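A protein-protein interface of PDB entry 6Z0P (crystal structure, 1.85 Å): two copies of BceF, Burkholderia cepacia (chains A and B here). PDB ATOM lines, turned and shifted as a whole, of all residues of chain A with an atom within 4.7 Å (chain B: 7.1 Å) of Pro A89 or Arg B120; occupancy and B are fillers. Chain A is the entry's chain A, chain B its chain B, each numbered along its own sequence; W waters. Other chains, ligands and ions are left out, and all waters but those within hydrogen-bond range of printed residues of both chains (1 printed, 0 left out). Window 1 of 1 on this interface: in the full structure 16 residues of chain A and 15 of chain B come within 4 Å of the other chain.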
ATOM      1  N   THR A  88      22.200   3.777  -3.797  1.00  0.00           N
ATOM      2  CA  THR A  88      21.078   4.467  -3.116  1.00  0.00           C
ATOM      3  C   THR A  88      21.239   5.975  -3.226  1.00  0.00           C
ATOM      4  O   THR A  88      22.303   6.460  -3.598  1.00  0.00           O
ATOM      5  CB  THR A  88      21.053   4.182  -1.608  1.00  0.00           C
ATOM      6  OG1 THR A  88      22.242   4.757  -1.062  1.00  0.00           O
ATOM      7  CG2 THR A  88      20.971   2.720  -1.225  1.00  0.00           C
ATOM      8  N   PRO A  89      20.211   6.766  -2.855  1.00  0.00           N
ATOM      9  CA  PRO A  89      20.389   8.197  -2.607  1.00  0.00           C
ATOM     10  C   PRO A  89      21.326   8.500  -1.429  1.00  0.00           C
ATOM     11  O   PRO A  89      21.555   7.620  -0.618  1.00  0.00           O
ATOM     12  CB  PRO A  89      18.983   8.693  -2.239  1.00  0.00           C
ATOM     13  CG  PRO A  89      18.050   7.664  -2.828  1.00  0.00           C
ATOM     14  CD  PRO A  89      18.807   6.356  -2.751  1.00  0.00           C
ATOM     15  N   GLY A  90      21.834   9.733  -1.363  1.00  0.00           N
ATOM     16  CA  GLY A  90      22.656  10.227  -0.238  1.00  0.00           C
ATOM     17  C   GLY A  90      24.132   9.916  -0.398  1.00  0.00           C
ATOM     18  O   GLY A  90      24.855  10.032   0.598  1.00  0.00           O
ATOM     19  N   ILE A  91      24.577   9.593  -1.613  1.00  0.00           N
ATOM     20  CA  ILE A  91      25.971   9.132  -1.886  1.00  0.00           C
ATOM     21  C   ILE A  91      26.809  10.282  -2.463  1.00  0.00           C
ATOM     22  O   ILE A  91      28.046  10.150  -2.482  1.00  0.00           O
ATOM     23  CB  ILE A  91      25.954   7.894  -2.804  1.00  0.00           C
ATOM     24  CG1 ILE A  91      25.436   8.222  -4.210  1.00  0.00           C
ATOM     25  CG2 ILE A  91      25.169   6.773  -2.135  1.00  0.00           C
ATOM     26  CD1 ILE A  91      25.328   7.040  -5.130  1.00  0.00           C
ATOM     27  N   ARG A 119      12.272  11.016  -9.986  1.00  0.00           N
ATOM     28  CA  ARG A 119      11.512  10.901  -8.707  1.00  0.00           C
ATOM     29  C   ARG A 119      11.934  11.993  -7.716  1.00  0.00           C
ATOM     30  O   ARG A 119      11.115  12.326  -6.842  1.00  0.00           O
ATOM     31  CB  ARG A 119      11.704   9.525  -8.059  1.00  0.00           C
ATOM     32  CG  ARG A 119      11.168   8.361  -8.884  1.00  0.00           C
ATOM     33  CD  ARG A 119      11.267   6.991  -8.221  1.00  0.00           C
ATOM     34  NE  ARG A 119      10.524   5.971  -8.953  1.00  0.00           N
ATOM     35  CZ  ARG A 119       9.200   5.862  -8.951  1.00  0.00           C
ATOM     36  NH1 ARG A 119       8.462   6.714  -8.259  1.00  0.00           N
ATOM     37  NH2 ARG A 119       8.609   4.909  -9.653  1.00  0.00           N
ATOM     38  N   ARG A 120      13.164  12.504  -7.809  1.00  0.00           N
ATOM     39  CA  ARG A 120      13.697  13.529  -6.867  1.00  0.00           C
ATOM     40  C   ARG A 120      14.035  14.804  -7.634  1.00  0.00           C
ATOM     41  O   ARG A 120      13.627  15.891  -7.180  1.00  0.00           O
ATOM     42  CB  ARG A 120      14.949  13.016  -6.162  1.00  0.00           C
ATOM     43  CG  ARG A 120      14.695  11.779  -5.318  1.00  0.00           C
ATOM     44  CD  ARG A 120      15.962  10.965  -5.307  1.00  0.00           C
ATOM     45  NE  ARG A 120      16.796  11.479  -4.242  1.00  0.00           N
ATOM     46  CZ  ARG A 120      18.115  11.587  -4.281  1.00  0.00           C
ATOM     47  NH1 ARG A 120      18.796  11.213  -5.350  1.00  0.00           N
ATOM     48  NH2 ARG A 120      18.752  12.085  -3.238  1.00  0.00           N
ATOM     49  N   ARG A 165       7.459  15.889 -11.726  1.00  0.00           N
ATOM     50  CA  ARG A 165       7.462  14.464 -11.316  1.00  0.00           C
ATOM     51  C   ARG A 165       6.293  13.740 -11.976  1.00  0.00           C
ATOM     52  O   ARG A 165       5.134  14.087 -11.750  1.00  0.00           O
ATOM     53  CB  ARG A 165       7.421  14.378  -9.796  1.00  0.00           C
ATOM     54  CG  ARG A 165       7.417  12.949  -9.303  1.00  0.00           C
ATOM     55  CD  ARG A 165       7.488  13.025  -7.812  1.00  0.00           C
ATOM     56  NE  ARG A 165       7.478  11.677  -7.302  1.00  0.00           N
ATOM     57  CZ  ARG A 165       7.730  11.357  -6.047  1.00  0.00           C
ATOM     58  NH1 ARG A 165       8.021  12.296  -5.162  1.00  0.00           N
ATOM     59  NH2 ARG A 165       7.687  10.090  -5.684  1.00  0.00           N
ATOM     60  N   PRO A 198      19.268   5.481  -9.133  1.00  0.00           N
ATOM     61  CA  PRO A 198      20.094   4.451  -8.513  1.00  0.00           C
ATOM     62  C   PRO A 198      19.657   3.070  -9.011  1.00  0.00           C
ATOM     63  O   PRO A 198      18.522   2.908  -9.368  1.00  0.00           O
ATOM     64  CB  PRO A 198      19.842   4.620  -7.010  1.00  0.00           C
ATOM     65  CG  PRO A 198      18.502   5.324  -6.914  1.00  0.00           C
ATOM     66  CD  PRO A 198      18.333   6.109  -8.197  1.00  0.00           C
ATOM     67  N   MET A 223      29.127   4.157   3.844  1.00  0.00           N
ATOM     68  CA  MET A 223      27.648   4.069   3.693  1.00  0.00           C
ATOM     69  C   MET A 223      27.197   2.676   3.256  1.00  0.00           C
ATOM     70  O   MET A 223      26.009   2.370   3.460  1.00  0.00           O
ATOM     71  CB  MET A 223      27.147   5.062   2.647  1.00  0.00           C
ATOM     72  CG  MET A 223      26.576   6.309   3.238  1.00  0.00           C
ATOM     73  SD  MET A 223      25.752   7.276   1.971  1.00  0.00           S
ATOM     74  CE  MET A 223      24.053   6.828   2.317  1.00  0.00           C
ATOM     75  N   THR B  88      11.313  -1.148  -3.134  1.00  0.00           N
ATOM     76  CA  THR B  88      11.574   0.020  -4.015  1.00  0.00           C
ATOM     77  C   THR B  88      10.352   0.927  -4.094  1.00  0.00           C
ATOM     78  O   THR B  88       9.276   0.579  -3.631  1.00  0.00           O
ATOM     79  CB  THR B  88      11.884  -0.395  -5.461  1.00  0.00           C
ATOM     80  OG1 THR B  88      10.727  -1.052  -5.983  1.00  0.00           O
ATOM     81  CG2 THR B  88      13.085  -1.301  -5.649  1.00  0.00           C
ATOM     82  N   PRO B  89      10.478   2.124  -4.707  1.00  0.00           N
ATOM     83  CA  PRO B  89       9.314   2.926  -5.077  1.00  0.00           C
ATOM     84  C   PRO B  89       8.576   2.306  -6.277  1.00  0.00           C
ATOM     85  O   PRO B  89       9.151   1.472  -6.935  1.00  0.00           O
ATOM     86  CB  PRO B  89       9.902   4.302  -5.443  1.00  0.00           C
ATOM     87  CG  PRO B  89      11.352   4.263  -5.003  1.00  0.00           C
ATOM     88  CD  PRO B  89      11.746   2.803  -4.981  1.00  0.00           C
ATOM     89  N   SER B  94       1.937   4.131  -1.524  1.00  0.00           N
ATOM     90  CA  SER B  94       1.098   5.331  -1.246  1.00  0.00           C
ATOM     91  C   SER B  94      -0.380   4.956  -1.365  1.00  0.00           C
ATOM     92  O   SER B  94      -1.150   5.281  -0.460  1.00  0.00           O
ATOM     93  CB  SER B  94       1.410   6.479  -2.167  1.00  0.00           C
ATOM     94  OG  SER B  94       2.775   6.849  -2.090  1.00  0.00           O
ATOM     95  N   ASP B 115       3.418  10.298   6.621  1.00  0.00           N
ATOM     96  CA  ASP B 115       4.309  10.140   5.450  1.00  0.00           C
ATOM     97  C   ASP B 115       5.747  10.277   5.952  1.00  0.00           C
ATOM     98  O   ASP B 115       6.181  11.418   6.176  1.00  0.00           O
ATOM     99  CB  ASP B 115       3.952  11.154   4.366  1.00  0.00           C
ATOM    100  CG  ASP B 115       4.664  10.889   3.059  1.00  0.00           C
ATOM    101  OD1 ASP B 115       5.540  10.008   3.034  1.00  0.00           O
ATOM    102  OD2 ASP B 115       4.330  11.564   2.081  1.00  0.00           O
ATOM    103  N   ASP B 117       8.435   9.051   4.340  1.00  0.00           N
ATOM    104  CA  ASP B 117       9.387   9.129   3.206  1.00  0.00           C
ATOM    105  C   ASP B 117       9.663  10.602   2.926  1.00  0.00           C
ATOM    106  O   ASP B 117       8.815  11.261   2.306  1.00  0.00           O
ATOM    107  CB  ASP B 117       8.879   8.426   1.952  1.00  0.00           C
ATOM    108  CG  ASP B 117      10.008   8.157   0.976  1.00  0.00           C
ATOM    109  OD1 ASP B 117      10.973   8.948   0.960  1.00  0.00           O
ATOM    110  OD2 ASP B 117       9.935   7.142   0.274  1.00  0.00           O
ATOM    111  N   MET B 118      10.800  11.105   3.386  1.00  0.00           N
ATOM    112  CA  MET B 118      11.073  12.559   3.326  1.00  0.00           C
ATOM    113  C   MET B 118      11.917  12.890   2.094  1.00  0.00           C
ATOM    114  O   MET B 118      12.370  14.043   1.995  1.00  0.00           O
ATOM    115  CB  MET B 118      11.751  13.022   4.613  1.00  0.00           C
ATOM    116  CG  MET B 118      10.755  13.101   5.743  1.00  0.00           C
ATOM    117  SD  MET B 118      11.458  13.687   7.283  1.00  0.00           S
ATOM    118  CE  MET B 118      12.790  12.507   7.495  1.00  0.00           C
ATOM    119  N   ARG B 119      12.099  11.931   1.186  1.00  0.00           N
ATOM    120  CA  ARG B 119      12.788  12.166  -0.107  1.00  0.00           C
ATOM    121  C   ARG B 119      11.769  12.168  -1.237  1.00  0.00           C
ATOM    122  O   ARG B 119      12.024  12.845  -2.240  1.00  0.00           O
ATOM    123  CB  ARG B 119      13.824  11.090  -0.418  1.00  0.00           C
ATOM    124  CG  ARG B 119      15.092  11.202   0.407  1.00  0.00           C
ATOM    125  CD  ARG B 119      16.105  10.201  -0.086  1.00  0.00           C
ATOM    126  NE  ARG B 119      17.201  10.030   0.850  1.00  0.00           N
ATOM    127  CZ  ARG B 119      18.300  10.770   0.857  1.00  0.00           C
ATOM    128  NH1 ARG B 119      18.449  11.749  -0.019  1.00  0.00           N
ATOM    129  NH2 ARG B 119      19.252  10.535   1.743  1.00  0.00           N
ATOM    130  N   ARG B 120      10.686  11.402  -1.120  1.00  0.00           N
ATOM    131  CA  ARG B 120       9.718  11.324  -2.242  1.00  0.00           C
ATOM    132  C   ARG B 120       8.287  11.156  -1.740  1.00  0.00           C
ATOM    133  O   ARG B 120       7.409  10.937  -2.590  1.00  0.00           O
ATOM    134  CB  ARG B 120      10.082  10.193  -3.214  1.00  0.00           C
ATOM    135  CG  ARG B 120      11.009   9.143  -2.625  1.00  0.00           C
ATOM    136  CD  ARG B 120      11.286   7.917  -3.467  1.00  0.00           C
ATOM    137  NE  ARG B 120      12.272   7.190  -2.688  1.00  0.00           N
ATOM    138  CZ  ARG B 120      13.582   7.293  -2.858  1.00  0.00           C
ATOM    139  NH1 ARG B 120      14.403   6.625  -2.065  1.00  0.00           N
ATOM    140  NH2 ARG B 120      14.068   8.043  -3.833  1.00  0.00           N
ATOM    141  N   GLY B 121       8.044  11.282  -0.437  1.00  0.00           N
ATOM    142  CA  GLY B 121       6.672  11.181   0.087  1.00  0.00           C
ATOM    143  C   GLY B 121       5.778  12.195  -0.600  1.00  0.00           C
ATOM    144  O   GLY B 121       6.172  13.370  -0.653  1.00  0.00           O
ATOM    145  N   LEU B 122       4.649  11.756  -1.159  1.00  0.00           N
ATOM    146  CA  LEU B 122       3.629  12.666  -1.746  1.00  0.00           C
ATOM    147  C   LEU B 122       2.243  12.241  -1.263  1.00  0.00           C
ATOM    148  O   LEU B 122       1.313  12.286  -2.078  1.00  0.00           O
ATOM    149  CB  LEU B 122       3.716  12.662  -3.279  1.00  0.00           C
ATOM    150  CG  LEU B 122       4.031  11.321  -3.942  1.00  0.00           C
ATOM    151  CD1 LEU B 122       2.895  10.326  -3.756  1.00  0.00           C
ATOM    152  CD2 LEU B 122       4.351  11.508  -5.419  1.00  0.00           C
ATOM    153  N   LEU B 123       2.099  11.859   0.009  1.00  0.00           N
ATOM    154  CA  LEU B 123       0.774  11.471   0.561  1.00  0.00           C
ATOM    155  C   LEU B 123      -0.110  12.715   0.686  1.00  0.00           C
ATOM    156  O   LEU B 123      -1.329  12.567   0.592  1.00  0.00           O
ATOM    157  CB  LEU B 123       0.922  10.757   1.907  1.00  0.00           C
ATOM    158  CG  LEU B 123       1.708   9.447   1.869  1.00  0.00           C
ATOM    159  CD1 LEU B 123       1.464   8.621   3.122  1.00  0.00           C
ATOM    160  CD2 LEU B 123       1.374   8.627   0.632  1.00  0.00           C
ATOM    161  N   ALA B 162       5.181  14.546   4.973  1.00  0.00           N
ATOM    162  CA  ALA B 162       6.650  14.411   5.069  1.00  0.00           C
ATOM    163  C   ALA B 162       7.290  15.769   5.394  1.00  0.00           C
ATOM    164  O   ALA B 162       8.388  15.760   5.959  1.00  0.00           O
ATOM    165  CB  ALA B 162       7.193  13.830   3.795  1.00  0.00           C
ATOM    166  N   ARG B 165      11.348  18.889   2.064  1.00  0.00           N
ATOM    167  CA  ARG B 165      12.437  17.904   1.874  1.00  0.00           C
ATOM    168  C   ARG B 165      13.659  18.397   2.650  1.00  0.00           C
ATOM    169  O   ARG B 165      14.128  19.511   2.412  1.00  0.00           O
ATOM    170  CB  ARG B 165      12.687  17.738   0.377  1.00  0.00           C
ATOM    171  CG  ARG B 165      13.625  16.590   0.048  1.00  0.00           C
ATOM    172  CD  ARG B 165      14.302  16.773  -1.289  1.00  0.00           C
ATOM    173  NE  ARG B 165      15.384  15.815  -1.420  1.00  0.00           N
ATOM    174  CZ  ARG B 165      15.312  14.672  -2.088  1.00  0.00           C
ATOM    175  NH1 ARG B 165      14.202  14.323  -2.720  1.00  0.00           N
ATOM    176  NH2 ARG B 165      16.365  13.880  -2.115  1.00  0.00           N
ATOM    177  N   PRO B 197      10.040   4.806   4.253  1.00  0.00           N
ATOM    178  CA  PRO B 197      10.868   4.735   3.059  1.00  0.00           C
ATOM    179  C   PRO B 197      11.196   3.283   2.740  1.00  0.00           C
ATOM    180  O   PRO B 197      11.225   2.432   3.623  1.00  0.00           O
ATOM    181  CB  PRO B 197      12.158   5.502   3.385  1.00  0.00           C
ATOM    182  CG  PRO B 197      11.971   6.062   4.780  1.00  0.00           C
ATOM    183  CD  PRO B 197      10.741   5.416   5.383  1.00  0.00           C
ATOM    184  N   PRO B 198      11.484   2.967   1.466  1.00  0.00           N
ATOM    185  CA  PRO B 198      11.774   1.593   1.071  1.00  0.00           C
ATOM    186  C   PRO B 198      13.073   1.108   1.717  1.00  0.00           C
ATOM    187  O   PRO B 198      13.946   1.912   1.987  1.00  0.00           O
ATOM    188  CB  PRO B 198      11.895   1.654  -0.455  1.00  0.00           C
ATOM    189  CG  PRO B 198      12.223   3.105  -0.752  1.00  0.00           C
ATOM    190  CD  PRO B 198      11.585   3.919   0.354  1.00  0.00           C
ATOM    191  N   LEU B 200      16.219  -0.029   1.291  1.00  0.00           N
ATOM    192  CA  LEU B 200      17.287  -0.136   0.266  1.00  0.00           C
ATOM    193  C   LEU B 200      18.591  -0.574   0.926  1.00  0.00           C
ATOM    194  O   LEU B 200      19.446  -1.107   0.219  1.00  0.00           O
ATOM    195  CB  LEU B 200      17.476   1.212  -0.432  1.00  0.00           C
ATOM    196  CG  LEU B 200      16.208   1.888  -0.949  1.00  0.00           C
ATOM    197  CD1 LEU B 200      16.532   3.228  -1.590  1.00  0.00           C
ATOM    198  CD2 LEU B 200      15.482   0.995  -1.937  1.00  0.00           C
ATOM    199  N   ASP B 204      18.163   1.930   6.334  1.00  0.00           N
ATOM    200  CA  ASP B 204      16.688   1.948   6.126  1.00  0.00           C
ATOM    201  C   ASP B 204      16.015   0.964   7.091  1.00  0.00           C
ATOM    202  O   ASP B 204      14.995   1.338   7.683  1.00  0.00           O
ATOM    203  CB  ASP B 204      16.316   1.659   4.675  1.00  0.00           C
ATOM    204  CG  ASP B 204      16.842   2.719   3.727  1.00  0.00           C
ATOM    205  OD1 ASP B 204      16.450   3.889   3.888  1.00  0.00           O
ATOM    206  OD2 ASP B 204      17.675   2.378   2.875  1.00  0.00           O
HETATM  207  O   HOH W   1      20.485  13.425  -1.001  1.00  0.00           O
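Of the 17 printed residues of chain B, 6 touch a printed residue of chain A.
Among the printed residues, 10 pairs touch across the chains.
The guanidinium group (NH1) of Arg A165 sits at hydrogen-bond distance from the backbone carbonyl oxygen (O) of Arg B120 (3.0 Å).
The guanidinium group (NH1) of Arg B119 sits close to the guanidinium group (NH2) of Arg A120 (3.3 Å).
The guanidinium group (NH2) of Arg A120 lies close to the guanidinium group (NH2) of Arg B165, at 3.2 Å.
Printed residues of chain B within 4 Å of Thr A88: Leu B200.
Pro A89 touches just these residues of chain B: Arg B119 and Arg B120.
Of the printed residues of chain B, Gly A90 touches Arg B119.
Of the printed residues of chain A, Leu B122 touches Arg A165.
Of the printed residues of chain A, Arg B165 touches Arg A120.
Of the printed residues of chain A, Leu B200 touches Thr A88 (3.9 Å).
The nearest residue of chain A that does not touch Arg B120 is Arg A119 (4.3 Å).
Pro A89 touches Arg B120, but with the chains exchanged Arg A120 does not touch Pro B89 (8.1 Å).
Arg A120 touches Arg B119, but with the chains exchanged Arg A119 does not touch Arg B120 (4.3 Å).
Arg B120 touches its own counterpart, Arg A120.
Arg A120 touches Arg B165, and with the chains exchanged Arg A165 touches Arg B120.
6 positions are printed for both chains.
Water W1 lies within hydrogen-bond range of the guanidinium group (NH1) of Arg B119 (2.8 Å) and the guanidinium group (NH2) of Arg A120 (3.1 Å).
OD2 of Asp B115 sits at hydrogen-bond distance from N of Leu B122 (3.3 Å).
The side-chain carboxylate (OD1) of Asp B117 sits at hydrogen-bond distance from the backbone NH (N) of Arg B119 (3.2 Å).
The side-chain carboxylate (OD2) of Asp B117 lies within salt-bridge range of the guanidinium group (NE) of Arg B120, at 3.8 Å.
The guanidinium group (NH1) of Arg B165 sits at hydrogen-bond distance from the backbone carbonyl oxygen (O) of Arg B119.
The backbone NH (N) of Leu B200 lies within hydrogen-bond range of the side-chain carboxylate (OD2) of Asp B204 (3.2 Å).
Among the printed residues, pairs that only touch across the chains: Thr A88 with Leu B200, Pro A89 with Arg B119, Pro A89 with Arg B120, Gly A90 with Arg B119, Arg A119 with Pro B89, Arg A120 with Arg B120 and Arg A165 with Leu B122.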
